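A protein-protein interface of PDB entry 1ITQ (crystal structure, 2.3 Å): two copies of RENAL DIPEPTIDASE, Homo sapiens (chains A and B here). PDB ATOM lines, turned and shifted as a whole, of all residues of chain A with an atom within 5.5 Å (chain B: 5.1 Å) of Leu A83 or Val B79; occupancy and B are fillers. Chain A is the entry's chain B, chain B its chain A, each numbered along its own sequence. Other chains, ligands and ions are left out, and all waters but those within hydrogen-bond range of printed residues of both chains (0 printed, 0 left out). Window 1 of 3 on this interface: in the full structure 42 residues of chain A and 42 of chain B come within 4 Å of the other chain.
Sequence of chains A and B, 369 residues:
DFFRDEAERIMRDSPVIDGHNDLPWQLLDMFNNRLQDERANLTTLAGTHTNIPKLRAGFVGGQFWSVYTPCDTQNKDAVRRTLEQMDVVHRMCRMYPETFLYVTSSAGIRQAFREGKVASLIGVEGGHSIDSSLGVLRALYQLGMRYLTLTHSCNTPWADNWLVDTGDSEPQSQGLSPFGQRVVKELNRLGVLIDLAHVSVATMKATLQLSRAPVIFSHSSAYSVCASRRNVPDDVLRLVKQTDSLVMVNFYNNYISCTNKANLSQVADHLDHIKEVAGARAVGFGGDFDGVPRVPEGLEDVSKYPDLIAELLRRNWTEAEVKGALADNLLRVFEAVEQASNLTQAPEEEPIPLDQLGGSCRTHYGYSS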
ATOM      1  N   ALA A  78       4.955 -21.729  -1.003  1.00  0.00           N
ATOM      2  CA  ALA A  78       5.981 -21.604   0.030  1.00  0.00           C
ATOM      3  C   ALA A  78       5.728 -20.495   1.031  1.00  0.00           C
ATOM      4  O   ALA A  78       5.947 -20.677   2.233  1.00  0.00           O
ATOM      5  CB  ALA A  78       7.351 -21.422  -0.611  1.00  0.00           C
ATOM      6  N   VAL A  79       5.269 -19.341   0.545  1.00  0.00           N
ATOM      7  CA  VAL A  79       5.027 -18.210   1.438  1.00  0.00           C
ATOM      8  C   VAL A  79       3.786 -18.426   2.300  1.00  0.00           C
ATOM      9  O   VAL A  79       3.813 -18.175   3.500  1.00  0.00           O
ATOM     10  CB  VAL A  79       4.962 -16.878   0.667  1.00  0.00           C
ATOM     11  CG1 VAL A  79       4.841 -15.727   1.626  1.00  0.00           C
ATOM     12  CG2 VAL A  79       6.204 -16.716  -0.179  1.00  0.00           C
ATOM     13  N   ARG A  80       2.720 -18.939   1.693  1.00  0.00           N
ATOM     14  CA  ARG A  80       1.478 -19.233   2.407  1.00  0.00           C
ATOM     15  C   ARG A  80       1.776 -20.178   3.561  1.00  0.00           C
ATOM     16  O   ARG A  80       1.536 -19.851   4.724  1.00  0.00           O
ATOM     17  CB  ARG A  80       0.497 -19.918   1.459  1.00  0.00           C
ATOM     18  CG  ARG A  80      -0.862 -20.231   2.063  1.00  0.00           C
ATOM     19  CD  ARG A  80      -1.530 -21.260   1.198  1.00  0.00           C
ATOM     20  NE  ARG A  80      -2.931 -21.471   1.525  1.00  0.00           N
ATOM     21  CZ  ARG A  80      -3.394 -22.499   2.227  1.00  0.00           C
ATOM     22  NH1 ARG A  80      -4.693 -22.602   2.457  1.00  0.00           N
ATOM     23  NH2 ARG A  80      -2.564 -23.407   2.721  1.00  0.00           N
ATOM     24  N   ARG A  81       2.351 -21.333   3.231  1.00  0.00           N
ATOM     25  CA  ARG A  81       2.689 -22.347   4.231  1.00  0.00           C
ATOM     26  C   ARG A  81       3.672 -21.879   5.302  1.00  0.00           C
ATOM     27  O   ARG A  81       3.589 -22.308   6.455  1.00  0.00           O
ATOM     28  CB  ARG A  81       3.173 -23.623   3.543  1.00  0.00           C
ATOM     29  CG  ARG A  81       2.086 -24.276   2.709  1.00  0.00           C
ATOM     30  CD  ARG A  81       2.390 -25.724   2.376  1.00  0.00           C
ATOM     31  NE  ARG A  81       1.228 -26.387   1.787  1.00  0.00           N
ATOM     32  CZ  ARG A  81       0.214 -26.898   2.486  1.00  0.00           C
ATOM     33  NH1 ARG A  81      -0.805 -27.473   1.857  1.00  0.00           N
ATOM     34  NH2 ARG A  81       0.223 -26.861   3.815  1.00  0.00           N
ATOM     35  N   THR A  82       4.574 -20.968   4.936  1.00  0.00           N
ATOM     36  CA  THR A  82       5.540 -20.424   5.890  1.00  0.00           C
ATOM     37  C   THR A  82       4.787 -19.659   6.958  1.00  0.00           C
ATOM     38  O   THR A  82       5.149 -19.701   8.132  1.00  0.00           O
ATOM     39  CB  THR A  82       6.537 -19.461   5.212  1.00  0.00           C
ATOM     40  OG1 THR A  82       7.238 -20.166   4.187  1.00  0.00           O
ATOM     41  CG2 THR A  82       7.545 -18.932   6.216  1.00  0.00           C
ATOM     42  N   LEU A  83       3.734 -18.962   6.538  1.00  0.00           N
ATOM     43  CA  LEU A  83       2.906 -18.183   7.452  1.00  0.00           C
ATOM     44  C   LEU A  83       2.084 -19.095   8.346  1.00  0.00           C
ATOM     45  O   LEU A  83       1.957 -18.853   9.551  1.00  0.00           O
ATOM     46  CB  LEU A  83       1.996 -17.230   6.671  1.00  0.00           C
ATOM     47  CG  LEU A  83       2.707 -16.125   5.878  1.00  0.00           C
ATOM     48  CD1 LEU A  83       1.672 -15.087   5.437  1.00  0.00           C
ATOM     49  CD2 LEU A  83       3.790 -15.455   6.733  1.00  0.00           C
ATOM     50  N   GLU A  84       1.554 -20.164   7.759  1.00  0.00           N
ATOM     51  CA  GLU A  84       0.757 -21.132   8.506  1.00  0.00           C
ATOM     52  C   GLU A  84       1.592 -21.799   9.572  1.00  0.00           C
ATOM     53  O   GLU A  84       1.171 -21.916  10.722  1.00  0.00           O
ATOM     54  CB  GLU A  84       0.194 -22.179   7.568  1.00  0.00           C
ATOM     55  CG  GLU A  84      -0.733 -21.585   6.546  1.00  0.00           C
ATOM     56  CD  GLU A  84      -1.494 -22.635   5.786  1.00  0.00           C
ATOM     57  OE1 GLU A  84      -0.883 -23.645   5.373  1.00  0.00           O
ATOM     58  OE2 GLU A  84      -2.714 -22.449   5.604  1.00  0.00           O
ATOM     59  N   GLN A  85       2.814 -22.167   9.198  1.00  0.00           N
ATOM     60  CA  GLN A  85       3.739 -22.816  10.114  1.00  0.00           C
ATOM     61  C   GLN A  85       4.201 -21.870  11.196  1.00  0.00           C
ATOM     62  O   GLN A  85       4.429 -22.288  12.333  1.00  0.00           O
ATOM     63  CB  GLN A  85       4.912 -23.416   9.349  1.00  0.00           C
ATOM     64  CG  GLN A  85       4.483 -24.540   8.415  1.00  0.00           C
ATOM     65  CD  GLN A  85       3.598 -25.575   9.113  1.00  0.00           C
ATOM     66  OE1 GLN A  85       2.410 -25.716   8.796  1.00  0.00           O
ATOM     67  NE2 GLN A  85       4.173 -26.292  10.073  1.00  0.00           N
ATOM     68  N   MET A  86       4.350 -20.591  10.854  1.00  0.00           N
ATOM     69  CA  MET A  86       4.739 -19.609  11.860  1.00  0.00           C
ATOM     70  C   MET A  86       3.530 -19.420  12.764  1.00  0.00           C
ATOM     71  O   MET A  86       3.669 -19.271  13.980  1.00  0.00           O
ATOM     72  CB  MET A  86       5.141 -18.277  11.221  1.00  0.00           C
ATOM     73  CG  MET A  86       6.450 -18.331  10.450  1.00  0.00           C
ATOM     74  SD  MET A  86       6.932 -16.745   9.764  1.00  0.00           S
ATOM     75  CE  MET A  86       7.860 -16.081  11.094  1.00  0.00           C
ATOM     76  N   ASP A  87       2.338 -19.486  12.172  1.00  0.00           N
ATOM     77  CA  ASP A  87       1.110 -19.337  12.944  1.00  0.00           C
ATOM     78  C   ASP A  87       0.979 -20.443  13.995  1.00  0.00           C
ATOM     79  O   ASP A  87       0.709 -20.163  15.164  1.00  0.00           O
ATOM     80  CB  ASP A  87      -0.111 -19.328  12.015  1.00  0.00           C
ATOM     81  CG  ASP A  87      -1.428 -19.270  12.776  1.00  0.00           C
ATOM     82  OD1 ASP A  87      -1.632 -18.320  13.558  1.00  0.00           O
ATOM     83  OD2 ASP A  87      -2.253 -20.190  12.595  1.00  0.00           O
ATOM     84  N   VAL A  88       1.216 -21.690  13.593  1.00  0.00           N
ATOM     85  CA  VAL A  88       1.112 -22.812  14.526  1.00  0.00           C
ATOM     86  C   VAL A  88       2.063 -22.653  15.717  1.00  0.00           C
ATOM     87  O   VAL A  88       1.697 -22.976  16.850  1.00  0.00           O
ATOM     88  CB  VAL A  88       1.296 -24.194  13.814  1.00  0.00           C
ATOM     89  CG1 VAL A  88       2.749 -24.509  13.580  1.00  0.00           C
ATOM     90  CG2 VAL A  88       0.640 -25.296  14.616  1.00  0.00           C
ATOM     91  N   LEU A 140       8.449 -11.582   7.423  1.00  0.00           N
ATOM     92  CA  LEU A 140       8.793 -12.737   8.244  1.00  0.00           C
ATOM     93  C   LEU A 140       9.544 -12.312   9.493  1.00  0.00           C
ATOM     94  O   LEU A 140       9.363 -12.890  10.564  1.00  0.00           O
ATOM     95  CB  LEU A 140       9.607 -13.750   7.436  1.00  0.00           C
ATOM     96  CG  LEU A 140       8.831 -14.361   6.269  1.00  0.00           C
ATOM     97  CD1 LEU A 140       9.548 -15.585   5.710  1.00  0.00           C
ATOM     98  CD2 LEU A 140       7.452 -14.748   6.749  1.00  0.00           C
ATOM     99  N   LEU A 143       7.104 -11.129  12.023  1.00  0.00           N
ATOM    100  CA  LEU A 143       6.312 -12.257  12.479  1.00  0.00           C
ATOM    101  C   LEU A 143       7.071 -13.217  13.393  1.00  0.00           C
ATOM    102  O   LEU A 143       6.531 -14.249  13.780  1.00  0.00           O
ATOM    103  CB  LEU A 143       5.731 -13.005  11.281  1.00  0.00           C
ATOM    104  CG  LEU A 143       4.667 -12.221  10.521  1.00  0.00           C
ATOM    105  CD1 LEU A 143       4.268 -12.968   9.282  1.00  0.00           C
ATOM    106  CD2 LEU A 143       3.463 -11.984  11.420  1.00  0.00           C
ATOM    107  N   ASP B  77       0.711 -15.528  -6.795  1.00  0.00           N
ATOM    108  CA  ASP B  77       1.584 -14.849  -5.850  1.00  0.00           C
ATOM    109  C   ASP B  77       0.871 -13.810  -4.997  1.00  0.00           C
ATOM    110  O   ASP B  77       1.497 -12.878  -4.486  1.00  0.00           O
ATOM    111  CB  ASP B  77       2.789 -14.227  -6.574  1.00  0.00           C
ATOM    112  CG  ASP B  77       2.398 -13.308  -7.727  1.00  0.00           C
ATOM    113  OD1 ASP B  77       3.274 -12.548  -8.173  1.00  0.00           O
ATOM    114  OD2 ASP B  77       1.247 -13.354  -8.210  1.00  0.00           O
ATOM    115  N   ALA B  78      -0.422 -14.017  -4.778  1.00  0.00           N
ATOM    116  CA  ALA B  78      -1.227 -13.091  -3.985  1.00  0.00           C
ATOM    117  C   ALA B  78      -0.688 -12.836  -2.592  1.00  0.00           C
ATOM    118  O   ALA B  78      -0.670 -11.694  -2.144  1.00  0.00           O
ATOM    119  CB  ALA B  78      -2.680 -13.578  -3.896  1.00  0.00           C
ATOM    120  N   VAL B  79      -0.252 -13.896  -1.911  1.00  0.00           N
ATOM    121  CA  VAL B  79       0.260 -13.786  -0.538  1.00  0.00           C
ATOM    122  C   VAL B  79       1.581 -13.038  -0.465  1.00  0.00           C
ATOM    123  O   VAL B  79       1.783 -12.202   0.414  1.00  0.00           O
ATOM    124  CB  VAL B  79       0.416 -15.176   0.130  1.00  0.00           C
ATOM    125  CG1 VAL B  79       0.861 -15.019   1.561  1.00  0.00           C
ATOM    126  CG2 VAL B  79      -0.898 -15.939   0.080  1.00  0.00           C
ATOM    127  N   ARG B  80       2.484 -13.360  -1.382  1.00  0.00           N
ATOM    128  CA  ARG B  80       3.785 -12.703  -1.444  1.00  0.00           C
ATOM    129  C   ARG B  80       3.591 -11.204  -1.714  1.00  0.00           C
ATOM    130  O   ARG B  80       4.108 -10.356  -0.984  1.00  0.00           O
ATOM    131  CB  ARG B  80       4.620 -13.313  -2.569  1.00  0.00           C
ATOM    132  CG  ARG B  80       5.975 -12.647  -2.777  1.00  0.00           C
ATOM    133  CD  ARG B  80       6.432 -12.877  -4.199  1.00  0.00           C
ATOM    134  NE  ARG B  80       7.863 -12.654  -4.388  1.00  0.00           N
ATOM    135  CZ  ARG B  80       8.373 -11.712  -5.174  1.00  0.00           C
ATOM    136  NH1 ARG B  80       9.684 -11.594  -5.310  1.00  0.00           N
ATOM    137  NH2 ARG B  80       7.572 -10.858  -5.793  1.00  0.00           N
ATOM    138  N   ARG B  81       2.839 -10.886  -2.765  1.00  0.00           N
ATOM    139  CA  ARG B  81       2.596  -9.492  -3.119  1.00  0.00           C
ATOM    140  C   ARG B  81       1.889  -8.726  -2.019  1.00  0.00           C
ATOM    141  O   ARG B  81       2.209  -7.566  -1.767  1.00  0.00           O
ATOM    142  CB  ARG B  81       1.864  -9.383  -4.454  1.00  0.00           C
ATOM    143  CG  ARG B  81       2.742  -9.822  -5.620  1.00  0.00           C
ATOM    144  CD  ARG B  81       2.244  -9.317  -6.965  1.00  0.00           C
ATOM    145  NE  ARG B  81       3.217  -9.568  -8.034  1.00  0.00           N
ATOM    146  CZ  ARG B  81       4.391  -8.951  -8.149  1.00  0.00           C
ATOM    147  NH1 ARG B  81       5.203  -9.254  -9.152  1.00  0.00           N
ATOM    148  NH2 ARG B  81       4.757  -8.023  -7.271  1.00  0.00           N
ATOM    149  N   THR B  82       0.972  -9.387  -1.320  1.00  0.00           N
ATOM    150  CA  THR B  82       0.272  -8.739  -0.216  1.00  0.00           C
ATOM    151  C   THR B  82       1.296  -8.320   0.833  1.00  0.00           C
ATOM    152  O   THR B  82       1.248  -7.199   1.331  1.00  0.00           O
ATOM    153  CB  THR B  82      -0.781  -9.683   0.431  1.00  0.00           C
ATOM    154  OG1 THR B  82      -1.780 -10.004  -0.537  1.00  0.00           O
ATOM    155  CG2 THR B  82      -1.448  -9.030   1.628  1.00  0.00           C
ATOM    156  N   LEU B  83       2.241  -9.209   1.145  1.00  0.00           N
ATOM    157  CA  LEU B  83       3.275  -8.902   2.144  1.00  0.00           C
ATOM    158  C   LEU B  83       4.178  -7.758   1.681  1.00  0.00           C
ATOM    159  O   LEU B  83       4.620  -6.932   2.488  1.00  0.00           O
ATOM    160  CB  LEU B  83       4.113 -10.144   2.474  1.00  0.00           C
ATOM    161  CG  LEU B  83       3.389 -11.375   3.031  1.00  0.00           C
ATOM    162  CD1 LEU B  83       4.411 -12.390   3.520  1.00  0.00           C
ATOM    163  CD2 LEU B  83       2.484 -10.973   4.173  1.00  0.00           C
ATOM    164  N   HIS B 128      -8.552 -13.002  -1.518  1.00  0.00           N
ATOM    165  CA  HIS B 128      -7.554 -13.856  -2.156  1.00  0.00           C
ATOM    166  C   HIS B 128      -6.146 -13.659  -1.595  1.00  0.00           C
ATOM    167  O   HIS B 128      -5.238 -14.433  -1.893  1.00  0.00           O
ATOM    168  CB  HIS B 128      -7.560 -13.648  -3.668  1.00  0.00           C
ATOM    169  CG  HIS B 128      -7.249 -12.248  -4.097  1.00  0.00           C
ATOM    170  ND1 HIS B 128      -8.174 -11.229  -4.040  1.00  0.00           N
ATOM    171  CD2 HIS B 128      -6.128 -11.709  -4.632  1.00  0.00           C
ATOM    172  CE1 HIS B 128      -7.637 -10.124  -4.523  1.00  0.00           C
ATOM    173  NE2 HIS B 128      -6.396 -10.389  -4.889  1.00  0.00           N
ATOM    174  N   SER B 129      -5.980 -12.616  -0.786  1.00  0.00           N
ATOM    175  CA  SER B 129      -4.710 -12.299  -0.154  1.00  0.00           C
ATOM    176  C   SER B 129      -4.378 -13.295   0.950  1.00  0.00           C
ATOM    177  O   SER B 129      -3.211 -13.451   1.308  1.00  0.00           O
ATOM    178  CB  SER B 129      -4.741 -10.890   0.443  1.00  0.00           C
ATOM    179  OG  SER B 129      -4.686  -9.900  -0.564  1.00  0.00           O
ATOM    180  N   ILE B 130      -5.399 -13.917   1.537  1.00  0.00           N
ATOM    181  CA  ILE B 130      -5.151 -14.888   2.592  1.00  0.00           C
ATOM    182  C   ILE B 130      -5.056 -16.302   2.030  1.00  0.00           C
ATOM    183  O   ILE B 130      -4.658 -17.229   2.731  1.00  0.00           O
ATOM    184  CB  ILE B 130      -6.223 -14.849   3.722  1.00  0.00           C
ATOM    185  CG1 ILE B 130      -7.545 -15.450   3.245  1.00  0.00           C
ATOM    186  CG2 ILE B 130      -6.400 -13.421   4.250  1.00  0.00           C
ATOM    187  CD1 ILE B 130      -8.484 -15.805   4.377  1.00  0.00           C
ATOM    188  N   ASP B 131      -5.388 -16.444   0.751  1.00  0.00           N
ATOM    189  CA  ASP B 131      -5.375 -17.736   0.059  1.00  0.00           C
ATOM    190  C   ASP B 131      -6.057 -18.833   0.891  1.00  0.00           C
ATOM    191  O   ASP B 131      -5.467 -19.877   1.167  1.00  0.00           O
ATOM    192  CB  ASP B 131      -3.939 -18.139  -0.304  1.00  0.00           C
ATOM    193  CG  ASP B 131      -3.889 -19.241  -1.349  1.00  0.00           C
ATOM    194  OD1 ASP B 131      -2.894 -19.991  -1.372  1.00  0.00           O
ATOM    195  OD2 ASP B 131      -4.832 -19.361  -2.155  1.00  0.00           O
ATOM    196  N   GLY B 135      -4.470 -19.048   9.029  1.00  0.00           N
ATOM    197  CA  GLY B 135      -3.140 -18.746   9.539  1.00  0.00           C
ATOM    198  C   GLY B 135      -2.517 -17.544   8.852  1.00  0.00           C
ATOM    199  O   GLY B 135      -1.791 -16.774   9.481  1.00  0.00           O
ATOM    200  N   VAL B 136      -2.750 -17.413   7.547  1.00  0.00           N
ATOM    201  CA  VAL B 136      -2.254 -16.259   6.808  1.00  0.00           C
ATOM    202  C   VAL B 136      -3.033 -15.050   7.336  1.00  0.00           C
ATOM    203  O   VAL B 136      -2.450 -13.998   7.603  1.00  0.00           O
ATOM    204  CB  VAL B 136      -2.474 -16.397   5.287  1.00  0.00           C
ATOM    205  CG1 VAL B 136      -2.083 -15.112   4.587  1.00  0.00           C
ATOM    206  CG2 VAL B 136      -1.644 -17.551   4.736  1.00  0.00           C
ATOM    207  N   ALA B 139      -1.635 -13.901  10.348  1.00  0.00           N
ATOM    208  CA  ALA B 139      -0.316 -13.339  10.079  1.00  0.00           C
ATOM    209  C   ALA B 139      -0.492 -11.897   9.595  1.00  0.00           C
ATOM    210  O   ALA B 139       0.195 -10.995  10.064  1.00  0.00           O
ATOM    211  CB  ALA B 139       0.417 -14.170   9.035  1.00  0.00           C
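Val A79 touches Leu B83, and with the chains exchanged Leu A83 touches Val B79. 6 positions are printed for both chains. Of the 8 pairs that touch across the chains among the printed residues, 2 have their exchanged pair printed and touching as well.
Printed residues of chain A that touch a printed residue of chain B: Val A79, Arg A80, Leu A83, Asp A87 and Leu A143. Among the printed residues, 8 pairs touch across the chains. Among the printed residues, Asp or Glu carboxylates within 4 Å of a Lys or Arg side-chain nitrogen of the other chain: Arg A80 with Asp B131 (3.3 Å).
The side-chain carboxylate of Asp B131 is in salt-bridge range of the guanidinium group of Arg A80 (3.3 Å).
The guanidinium group (NH2) of Arg A80 is in salt-bridge range of the side-chain carboxylate (OE2) of Glu A84, 3.0 Å away.
Of chain B, only Val B79, Val B136 and Ala B139 come within 4 Å of Leu A83. Val B79 touches just one residue of chain A: Leu A83 (3.96 Å). Printed residues of chain B within 4 Å of Val A79: Leu B83. Of the printed residues of chain B, Arg A80 touches Asp B131 (3.0 Å) and Val B136 (3.9 Å). His B128 touches none of the printed residues of chain A. The nearest residue of chain A that does not touch Val B79 is Val A79 (4.04 Å). The nearest printed residue of chain B that does not touch Val A79 is Val B79 (4.04 Å).
Val A79 touches Leu B83. Arg A80 touches Val B136. Leu A83 touches Val B79. CD1 of Leu A83 touches CG1 of Val B136, at 3.9 Å. Ala B139 touches Leu A83 (CB to CD1, 3.9 Å). Asp A87 touches Gly B135 (OD2 to CA, 3.5 Å). Leu A143 touches Ala B139.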
